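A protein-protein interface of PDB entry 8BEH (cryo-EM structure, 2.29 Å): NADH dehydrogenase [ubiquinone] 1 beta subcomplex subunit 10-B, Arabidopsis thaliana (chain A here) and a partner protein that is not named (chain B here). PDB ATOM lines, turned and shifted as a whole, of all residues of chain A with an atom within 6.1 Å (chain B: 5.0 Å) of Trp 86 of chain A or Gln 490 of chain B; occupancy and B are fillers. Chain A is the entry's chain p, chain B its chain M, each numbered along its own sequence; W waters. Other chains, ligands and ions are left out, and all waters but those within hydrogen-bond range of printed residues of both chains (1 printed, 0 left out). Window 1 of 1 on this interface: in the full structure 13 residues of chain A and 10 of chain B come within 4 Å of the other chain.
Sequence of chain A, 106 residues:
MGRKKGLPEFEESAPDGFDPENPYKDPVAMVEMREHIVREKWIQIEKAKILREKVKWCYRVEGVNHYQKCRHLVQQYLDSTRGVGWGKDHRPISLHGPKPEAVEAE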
ATOM      1  N   ARG A  34     -15.602  33.744 -22.504  1.00  0.00           N
ATOM      2  CA  ARG A  34     -15.739  32.574 -23.366  1.00  0.00           C
ATOM      3  C   ARG A  34     -16.417  31.422 -22.626  1.00  0.00           C
ATOM      4  O   ARG A  34     -17.343  30.787 -23.149  1.00  0.00           O
ATOM      5  CB  ARG A  34     -14.374  32.143 -23.902  1.00  0.00           C
ATOM      6  CG  ARG A  34     -14.454  31.046 -24.946  1.00  0.00           C
ATOM      7  CD  ARG A  34     -13.134  30.317 -25.110  1.00  0.00           C
ATOM      8  NE  ARG A  34     -12.883  29.405 -24.005  1.00  0.00           N
ATOM      9  CZ  ARG A  34     -11.719  29.286 -23.379  1.00  0.00           C
ATOM     10  NH1 ARG A  34     -10.669  30.001 -23.737  1.00  0.00           N
ATOM     11  NH2 ARG A  34     -11.611  28.431 -22.369  1.00  0.00           N
ATOM     12  N   ILE A  37     -20.162  32.223 -22.095  1.00  0.00           N
ATOM     13  CA  ILE A  37     -20.927  32.066 -23.329  1.00  0.00           C
ATOM     14  C   ILE A  37     -21.156  30.592 -23.628  1.00  0.00           C
ATOM     15  O   ILE A  37     -22.242  30.193 -24.066  1.00  0.00           O
ATOM     16  CB  ILE A  37     -20.213  32.779 -24.492  1.00  0.00           C
ATOM     17  CG1 ILE A  37     -20.319  34.297 -24.339  1.00  0.00           C
ATOM     18  CG2 ILE A  37     -20.764  32.322 -25.835  1.00  0.00           C
ATOM     19  CD1 ILE A  37     -19.283  35.050 -25.131  1.00  0.00           C
ATOM     20  N   VAL A  38     -20.135  29.758 -23.400  1.00  0.00           N
ATOM     21  CA  VAL A  38     -20.300  28.323 -23.611  1.00  0.00           C
ATOM     22  C   VAL A  38     -21.392  27.777 -22.699  1.00  0.00           C
ATOM     23  O   VAL A  38     -22.266  27.009 -23.132  1.00  0.00           O
ATOM     24  CB  VAL A  38     -18.959  27.593 -23.398  1.00  0.00           C
ATOM     25  CG1 VAL A  38     -19.183  26.108 -23.160  1.00  0.00           C
ATOM     26  CG2 VAL A  38     -18.042  27.811 -24.579  1.00  0.00           C
ATOM     27  N   LYS A  41     -24.829  28.941 -23.982  1.00  0.00           N
ATOM     28  CA  LYS A  41     -25.159  28.123 -25.150  1.00  0.00           C
ATOM     29  C   LYS A  41     -25.663  26.724 -24.751  1.00  0.00           C
ATOM     30  O   LYS A  41     -26.629  26.309 -25.345  1.00  0.00           O
ATOM     31  CB  LYS A  41     -24.046  28.175 -26.214  1.00  0.00           C
ATOM     32  CG  LYS A  41     -23.886  29.499 -26.931  1.00  0.00           C
ATOM     33  CD  LYS A  41     -22.789  29.491 -27.950  1.00  0.00           C
ATOM     34  CE  LYS A  41     -22.708  30.796 -28.704  1.00  0.00           C
ATOM     35  NZ  LYS A  41     -22.068  30.648 -30.026  1.00  0.00           N
ATOM     36  N   TRP A  42     -25.058  26.076 -23.760  1.00  0.00           N
ATOM     37  CA  TRP A  42     -25.537  24.777 -23.261  1.00  0.00           C
ATOM     38  C   TRP A  42     -26.940  24.908 -22.606  1.00  0.00           C
ATOM     39  O   TRP A  42     -27.698  23.991 -22.761  1.00  0.00           O
ATOM     40  CB  TRP A  42     -24.520  24.069 -22.363  1.00  0.00           C
ATOM     41  CG  TRP A  42     -23.498  23.358 -23.187  1.00  0.00           C
ATOM     42  CD1 TRP A  42     -22.239  23.782 -23.470  1.00  0.00           C
ATOM     43  CD2 TRP A  42     -23.672  22.118 -23.885  1.00  0.00           C
ATOM     44  NE1 TRP A  42     -21.604  22.877 -24.256  1.00  0.00           N
ATOM     45  CE2 TRP A  42     -22.454  21.851 -24.542  1.00  0.00           C
ATOM     46  CE3 TRP A  42     -24.724  21.210 -24.013  1.00  0.00           C
ATOM     47  CZ2 TRP A  42     -22.261  20.711 -25.317  1.00  0.00           C
ATOM     48  CZ3 TRP A  42     -24.535  20.085 -24.780  1.00  0.00           C
ATOM     49  CH2 TRP A  42     -23.317  19.835 -25.415  1.00  0.00           C
ATOM     50  N   ILE A  45     -29.305  24.814 -25.510  1.00  0.00           N
ATOM     51  CA  ILE A  45     -29.382  23.448 -26.057  1.00  0.00           C
ATOM     52  C   ILE A  45     -30.307  22.618 -25.152  1.00  0.00           C
ATOM     53  O   ILE A  45     -31.235  22.042 -25.698  1.00  0.00           O
ATOM     54  CB  ILE A  45     -28.003  22.801 -26.324  1.00  0.00           C
ATOM     55  CG1 ILE A  45     -27.215  23.556 -27.398  1.00  0.00           C
ATOM     56  CG2 ILE A  45     -28.116  21.316 -26.632  1.00  0.00           C
ATOM     57  CD1 ILE A  45     -25.743  23.672 -27.088  1.00  0.00           C
ATOM     58  N   VAL A  84     -29.269  27.471 -32.440  1.00  0.00           N
ATOM     59  CA  VAL A  84     -29.046  26.718 -31.188  1.00  0.00           C
ATOM     60  C   VAL A  84     -27.634  26.171 -31.328  1.00  0.00           C
ATOM     61  O   VAL A  84     -27.222  25.920 -32.428  1.00  0.00           O
ATOM     62  CB  VAL A  84     -30.093  25.603 -30.904  1.00  0.00           C
ATOM     63  CG1 VAL A  84     -29.904  24.355 -31.748  1.00  0.00           C
ATOM     64  CG2 VAL A  84     -30.174  25.277 -29.426  1.00  0.00           C
ATOM     65  N   GLY A  85     -26.946  26.045 -30.246  1.00  0.00           N
ATOM     66  CA  GLY A  85     -25.558  25.549 -30.239  1.00  0.00           C
ATOM     67  C   GLY A  85     -24.664  26.084 -31.310  1.00  0.00           C
ATOM     68  O   GLY A  85     -24.743  27.234 -31.627  1.00  0.00           O
ATOM     69  N   TRP A  86     -23.977  25.185 -31.962  1.00  0.00           N
ATOM     70  CA  TRP A  86     -22.956  25.605 -32.925  1.00  0.00           C
ATOM     71  C   TRP A  86     -23.259  24.987 -34.300  1.00  0.00           C
ATOM     72  O   TRP A  86     -22.355  24.955 -35.108  1.00  0.00           O
ATOM     73  CB  TRP A  86     -21.616  25.248 -32.291  1.00  0.00           C
ATOM     74  CG  TRP A  86     -21.206  25.961 -31.039  1.00  0.00           C
ATOM     75  CD1 TRP A  86     -20.426  27.072 -30.967  1.00  0.00           C
ATOM     76  CD2 TRP A  86     -21.457  25.570 -29.677  1.00  0.00           C
ATOM     77  NE1 TRP A  86     -20.197  27.418 -29.666  1.00  0.00           N
ATOM     78  CE2 TRP A  86     -20.816  26.516 -28.849  1.00  0.00           C
ATOM     79  CE3 TRP A  86     -22.188  24.546 -29.072  1.00  0.00           C
ATOM     80  CZ2 TRP A  86     -20.871  26.455 -27.459  1.00  0.00           C
ATOM     81  CZ3 TRP A  86     -22.226  24.473 -27.702  1.00  0.00           C
ATOM     82  CH2 TRP A  86     -21.580  25.417 -26.905  1.00  0.00           C
ATOM     83  N   GLY A  87     -24.563  24.791 -34.618  1.00  0.00           N
ATOM     84  CA  GLY A  87     -24.960  24.214 -35.887  1.00  0.00           C
ATOM     85  C   GLY A  87     -25.019  25.203 -37.036  1.00  0.00           C
ATOM     86  O   GLY A  87     -24.092  25.994 -37.228  1.00  0.00           O
ATOM     87  N   LYS A  88     -26.108  25.181 -37.800  1.00  0.00           N
ATOM     88  CA  LYS A  88     -26.178  25.880 -39.077  1.00  0.00           C
ATOM     89  C   LYS A  88     -26.579  27.349 -38.958  1.00  0.00           C
ATOM     90  O   LYS A  88     -26.839  27.984 -39.983  1.00  0.00           O
ATOM     91  CB  LYS A  88     -27.145  25.162 -40.019  1.00  0.00           C
ATOM     92  CG  LYS A  88     -26.652  25.082 -41.446  1.00  0.00           C
ATOM     93  CD  LYS A  88     -27.561  24.232 -42.305  1.00  0.00           C
ATOM     94  CE  LYS A  88     -27.690  24.814 -43.693  1.00  0.00           C
ATOM     95  NZ  LYS A  88     -28.524  23.973 -44.581  1.00  0.00           N
ATOM     96  N   ASP A  89     -26.566  27.926 -37.737  1.00  0.00           N
ATOM     97  CA  ASP A  89     -27.014  29.326 -37.429  1.00  0.00           C
ATOM     98  C   ASP A  89     -25.986  29.964 -36.491  1.00  0.00           C
ATOM     99  O   ASP A  89     -25.636  29.333 -35.483  1.00  0.00           O
ATOM    100  CB  ASP A  89     -28.436  29.303 -36.851  1.00  0.00           C
ATOM    101  CG  ASP A  89     -29.579  29.006 -37.814  1.00  0.00           C
ATOM    102  OD1 ASP A  89     -29.331  28.435 -38.887  1.00  0.00           O
ATOM    103  OD2 ASP A  89     -30.730  29.352 -37.474  1.00  0.00           O
ATOM    104  N   LEU B 326     -15.448  22.523 -37.166  1.00  0.00           N
ATOM    105  CA  LEU B 326     -15.545  23.526 -36.100  1.00  0.00           C
ATOM    106  C   LEU B 326     -16.944  23.588 -35.474  1.00  0.00           C
ATOM    107  O   LEU B 326     -17.519  24.660 -35.292  1.00  0.00           O
ATOM    108  CB  LEU B 326     -15.116  24.909 -36.607  1.00  0.00           C
ATOM    109  CG  LEU B 326     -13.730  25.419 -36.199  1.00  0.00           C
ATOM    110  CD1 LEU B 326     -13.592  25.498 -34.684  1.00  0.00           C
ATOM    111  CD2 LEU B 326     -12.623  24.559 -36.801  1.00  0.00           C
ATOM    112  N   ASN B 327     -17.488  22.424 -35.128  1.00  0.00           N
ATOM    113  CA  ASN B 327     -18.692  22.346 -34.308  1.00  0.00           C
ATOM    114  C   ASN B 327     -18.577  21.133 -33.394  1.00  0.00           C
ATOM    115  O   ASN B 327     -17.628  20.353 -33.486  1.00  0.00           O
ATOM    116  CB  ASN B 327     -19.979  22.285 -35.157  1.00  0.00           C
ATOM    117  CG  ASN B 327     -19.868  21.336 -36.335  1.00  0.00           C
ATOM    118  OD1 ASN B 327     -19.519  20.171 -36.178  1.00  0.00           O
ATOM    119  ND2 ASN B 327     -20.179  21.833 -37.520  1.00  0.00           N
ATOM    120  N   ILE B 328     -19.598  20.847 -32.569  1.00  0.00           N
ATOM    121  CA  ILE B 328     -19.540  19.772 -31.521  1.00  0.00           C
ATOM    122  C   ILE B 328     -19.460  18.387 -32.138  1.00  0.00           C
ATOM    123  O   ILE B 328     -18.563  17.691 -31.770  1.00  0.00           O
ATOM    124  CB  ILE B 328     -20.632  19.845 -30.407  1.00  0.00           C
ATOM    125  CG1 ILE B 328     -20.929  21.285 -29.969  1.00  0.00           C
ATOM    126  CG2 ILE B 328     -20.280  18.947 -29.235  1.00  0.00           C
ATOM    127  CD1 ILE B 328     -19.827  21.966 -29.210  1.00  0.00           C
ATOM    128  N   SER B 486     -16.380  22.235 -26.416  1.00  0.00           N
ATOM    129  CA  SER B 486     -17.198  23.433 -26.556  1.00  0.00           C
ATOM    130  C   SER B 486     -16.352  24.689 -26.471  1.00  0.00           C
ATOM    131  O   SER B 486     -16.536  25.623 -27.255  1.00  0.00           O
ATOM    132  CB  SER B 486     -18.283  23.451 -25.481  1.00  0.00           C
ATOM    133  OG  SER B 486     -19.324  22.553 -25.791  1.00  0.00           O
ATOM    134  N   ASN B 487     -15.419  24.735 -25.523  1.00  0.00           N
ATOM    135  CA  ASN B 487     -14.593  25.929 -25.406  1.00  0.00           C
ATOM    136  C   ASN B 487     -13.637  26.060 -26.587  1.00  0.00           C
ATOM    137  O   ASN B 487     -13.348  27.180 -27.022  1.00  0.00           O
ATOM    138  CB  ASN B 487     -13.856  25.925 -24.069  1.00  0.00           C
ATOM    139  CG  ASN B 487     -14.645  26.639 -22.979  1.00  0.00           C
ATOM    140  OD1 ASN B 487     -14.463  27.826 -22.737  1.00  0.00           O
ATOM    141  ND2 ASN B 487     -15.551  25.912 -22.339  1.00  0.00           N
ATOM    142  N   LEU B 488     -13.161  24.939 -27.137  1.00  0.00           N
ATOM    143  CA  LEU B 488     -12.368  24.994 -28.364  1.00  0.00           C
ATOM    144  C   LEU B 488     -13.179  25.554 -29.526  1.00  0.00           C
ATOM    145  O   LEU B 488     -12.680  26.372 -30.305  1.00  0.00           O
ATOM    146  CB  LEU B 488     -11.835  23.603 -28.708  1.00  0.00           C
ATOM    147  CG  LEU B 488     -10.935  23.447 -29.938  1.00  0.00           C
ATOM    148  CD1 LEU B 488      -9.784  24.450 -29.944  1.00  0.00           C
ATOM    149  CD2 LEU B 488     -10.410  22.013 -30.032  1.00  0.00           C
ATOM    150  N   VAL B 489     -14.432  25.122 -29.656  1.00  0.00           N
ATOM    151  CA  VAL B 489     -15.267  25.569 -30.764  1.00  0.00           C
ATOM    152  C   VAL B 489     -15.560  27.061 -30.647  1.00  0.00           C
ATOM    153  O   VAL B 489     -15.611  27.777 -31.650  1.00  0.00           O
ATOM    154  CB  VAL B 489     -16.559  24.729 -30.816  1.00  0.00           C
ATOM    155  CG1 VAL B 489     -17.659  25.469 -31.516  1.00  0.00           C
ATOM    156  CG2 VAL B 489     -16.303  23.411 -31.504  1.00  0.00           C
ATOM    157  N   GLN B 490     -15.738  27.556 -29.424  1.00  0.00           N
ATOM    158  CA  GLN B 490     -16.124  28.946 -29.236  1.00  0.00           C
ATOM    159  C   GLN B 490     -14.941  29.910 -29.257  1.00  0.00           C
ATOM    160  O   GLN B 490     -15.142  31.103 -29.511  1.00  0.00           O
ATOM    161  CB  GLN B 490     -16.912  29.087 -27.932  1.00  0.00           C
ATOM    162  CG  GLN B 490     -17.358  30.496 -27.601  1.00  0.00           C
ATOM    163  CD  GLN B 490     -18.599  30.895 -28.371  1.00  0.00           C
ATOM    164  OE1 GLN B 490     -19.548  30.123 -28.486  1.00  0.00           O
ATOM    165  NE2 GLN B 490     -18.603  32.111 -28.890  1.00  0.00           N
ATOM    166  N   HIS B 491     -13.723  29.421 -29.047  1.00  0.00           N
ATOM    167  CA  HIS B 491     -12.572  30.302 -28.884  1.00  0.00           C
ATOM    168  C   HIS B 491     -12.401  31.223 -30.087  1.00  0.00           C
ATOM    169  O   HIS B 491     -12.411  30.778 -31.237  1.00  0.00           O
ATOM    170  CB  HIS B 491     -11.307  29.471 -28.668  1.00  0.00           C
ATOM    171  CG  HIS B 491     -10.134  30.275 -28.212  1.00  0.00           C
ATOM    172  ND1 HIS B 491      -9.616  30.179 -26.938  1.00  0.00           N
ATOM    173  CD2 HIS B 491      -9.379  31.194 -28.856  1.00  0.00           C
ATOM    174  CE1 HIS B 491      -8.593  31.003 -26.819  1.00  0.00           C
ATOM    175  NE2 HIS B 491      -8.428  31.633 -27.967  1.00  0.00           N
ATOM    176  N   GLY B 492     -12.245  32.515 -29.811  1.00  0.00           N
ATOM    177  CA  GLY B 492     -12.098  33.522 -30.840  1.00  0.00           C
ATOM    178  C   GLY B 492     -13.355  34.305 -31.157  1.00  0.00           C
ATOM    179  O   GLY B 492     -13.267  35.321 -31.853  1.00  0.00           O
ATOM    180  N   LYS B 493     -14.515  33.866 -30.679  1.00  0.00           N
ATOM    181  CA  LYS B 493     -15.778  34.551 -30.906  1.00  0.00           C
ATOM    182  C   LYS B 493     -16.459  34.837 -29.577  1.00  0.00           C
ATOM    183  O   LYS B 493     -16.230  34.143 -28.582  1.00  0.00           O
ATOM    184  CB  LYS B 493     -16.710  33.725 -31.796  1.00  0.00           C
ATOM    185  CG  LYS B 493     -15.993  32.921 -32.846  1.00  0.00           C
ATOM    186  CD  LYS B 493     -16.648  31.586 -33.058  1.00  0.00           C
ATOM    187  CE  LYS B 493     -15.627  30.539 -33.451  1.00  0.00           C
ATOM    188  NZ  LYS B 493     -14.666  30.280 -32.353  1.00  0.00           N
ATOM    189  N   PHE B 494     -17.303  35.864 -29.563  1.00  0.00           N
ATOM    190  CA  PHE B 494     -17.980  36.274 -28.339  1.00  0.00           C
ATOM    191  C   PHE B 494     -19.462  36.513 -28.579  1.00  0.00           C
ATOM    192  O   PHE B 494     -20.061  37.431 -28.013  1.00  0.00           O
ATOM    193  CB  PHE B 494     -17.311  37.505 -27.740  1.00  0.00           C
ATOM    194  CG  PHE B 494     -15.862  37.302 -27.455  1.00  0.00           C
ATOM    195  CD1 PHE B 494     -15.457  36.620 -26.320  1.00  0.00           C
ATOM    196  CD2 PHE B 494     -14.903  37.751 -28.340  1.00  0.00           C
ATOM    197  CE1 PHE B 494     -14.117  36.413 -26.069  1.00  0.00           C
ATOM    198  CE2 PHE B 494     -13.573  37.546 -28.094  1.00  0.00           C
ATOM    199  CZ  PHE B 494     -13.178  36.875 -26.960  1.00  0.00           C
ATOM    200  N   HIS B 495     -20.082  35.677 -29.403  1.00  0.00           N
ATOM    201  CA  HIS B 495     -21.530  35.706 -29.566  1.00  0.00           C
ATOM    202  C   HIS B 495     -22.044  34.301 -29.845  1.00  0.00           C
ATOM    203  O   HIS B 495     -21.260  33.389 -30.101  1.00  0.00           O
ATOM    204  CB  HIS B 495     -21.939  36.672 -30.686  1.00  0.00           C
ATOM    205  CG  HIS B 495     -21.423  36.293 -32.036  1.00  0.00           C
ATOM    206  ND1 HIS B 495     -21.842  35.164 -32.708  1.00  0.00           N
ATOM    207  CD2 HIS B 495     -20.494  36.878 -32.827  1.00  0.00           C
ATOM    208  CE1 HIS B 495     -21.206  35.080 -33.862  1.00  0.00           C
ATOM    209  NE2 HIS B 495     -20.382  36.108 -33.958  1.00  0.00           N
HETATM  210  O   HOH W   1     -22.034  24.206 -37.990  1.00  0.00           O
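Of the printed residues of chain B, Val 38 of chain A touches Ser 486, Asn 487 and Gln 490. Of chain B, only Asn 327, Ile 328, Ser 486, Val 489 and Gln 490 come within 4 Å of Trp 86 of chain A. Asp 89 of chain A touches none of the printed residues of chain B. Leu 488 of chain B touches none of the printed residues of chain A. Of the printed residues of chain A, Val 489 of chain B touches Trp 86. Gln 490 of chain B touches five residues of chain A. The nearest residue of chain B that does not touch Trp 86 of chain A is Leu 326 of chain B (4.8 Å). The nearest printed residue of chain A that does not touch Gln 490 of chain B is Gly 85 of chain A (6.7 Å). The nearest printed residue of chain A that does not touch Val 489 of chain B is Val 38 of chain A (6.6 Å).
Printed residues of chain A that touch a printed residue of chain B: Arg 34, Ile 37, Val 38, Lys 41, Trp 42 and Trp 86. Hydrophobic or aromatic side chains of chain A within 4 Å of the printed part of chain B: Ile 37, Val 38, Trp 42 and Trp 86. Along chain A the printed residues that touch a printed residue of chain B span positions 34 to 86. Printed residues of chain B that touch a printed residue of chain A: Asn 327, Ile 328, Ser 486, Asn 487, Val 489, Gln 490, His 491, Phe 494 and His 495. Hydrophobic or aromatic side chains of chain B within 4 Å of the printed part of chain A: Ile 328, Val 489 and His 491. Among the printed residues, 16 pairs touch across the chains. Among the printed residues, no Asp or Glu carboxylate lies within 4 Å of a Lys or Arg side-chain nitrogen of the other chain.
Among the printed residues, merely in contact across the chains: Trp 86 of chain A with Val 489 of chain B (3.2 Å), Trp 86 of chain A with Ile 328 of chain B (3.5 Å), Trp 86 of chain A with Asn 327 of chain B (3.6 Å), Ile 37 of chain A with Gln 490 of chain B (3.6 Å), Val 38 of chain A with Ser 486 of chain B (3.6 Å), Ile 37 of chain A with Phe 494 of chain B (3.7 Å), Val 38 of chain A with Asn 487 of chain B (3.7 Å), Val 38 of chain A with Gln 490 of chain B (3.8 Å), Trp 86 of chain A with Ser 486 of chain B (3.8 Å) and Arg 34 of chain A with Gln 490 of chain B (3.97 Å).
The side-chain amino group of Lys 493 of chain B lies within hydrogen-bond range of the backbone carbonyl oxygen of Val 489 of chain B (2.8 Å). The side-chain amino group of Lys 493 of chain B lies within hydrogen-bond range of the backbone carbonyl oxygen of Gln 490 of chain B, 3.0 Å away. The side-chain amide nitrogen of Gln 490 of chain B is in hydrogen-bond range of the backbone carbonyl oxygen of His 495 of chain B (3.2 Å). NZ of Lys 493 of chain B lies within hydrogen-bond range of O of His 491 of chain B (2.6 Å).
Water W1 lies within hydrogen-bond range of the backbone carbonyl oxygen of Gly 87 of chain A (2.8 Å), the backbone carbonyl oxygen of Trp 86 of chain A (3.0 Å) and the side-chain amide nitrogen of Asn 327 of chain B (3.0 Å).
NE of Arg 34 of chain A sits at hydrogen-bond distance from OD1 of Asn 487 of chain B (2.6 Å). The guanidinium group of Arg 34 of chain A sits at hydrogen-bond distance from a ring nitrogen (ND1) of His 491 of chain B, at 3.4 Å. The side-chain amino group (NZ) of Lys 41 of chain A lies within hydrogen-bond range of the side-chain amide oxygen (OE1) of Gln 490 of chain B (3.0 Å). NZ of Lys 41 of chain A lies within hydrogen-bond range of O of His 495 of chain B (2.9 Å). The indole nitrogen (NE1) of Trp 42 of chain A lies within hydrogen-bond range of the side-chain hydroxyl (OG) of Ser 486 of chain B, at 2.8 Å. The indole nitrogen (NE1) of Trp 86 of chain A lies within hydrogen-bond range of the side-chain amide oxygen (OE1) of Gln 490 of chain B, 3.0 Å away.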
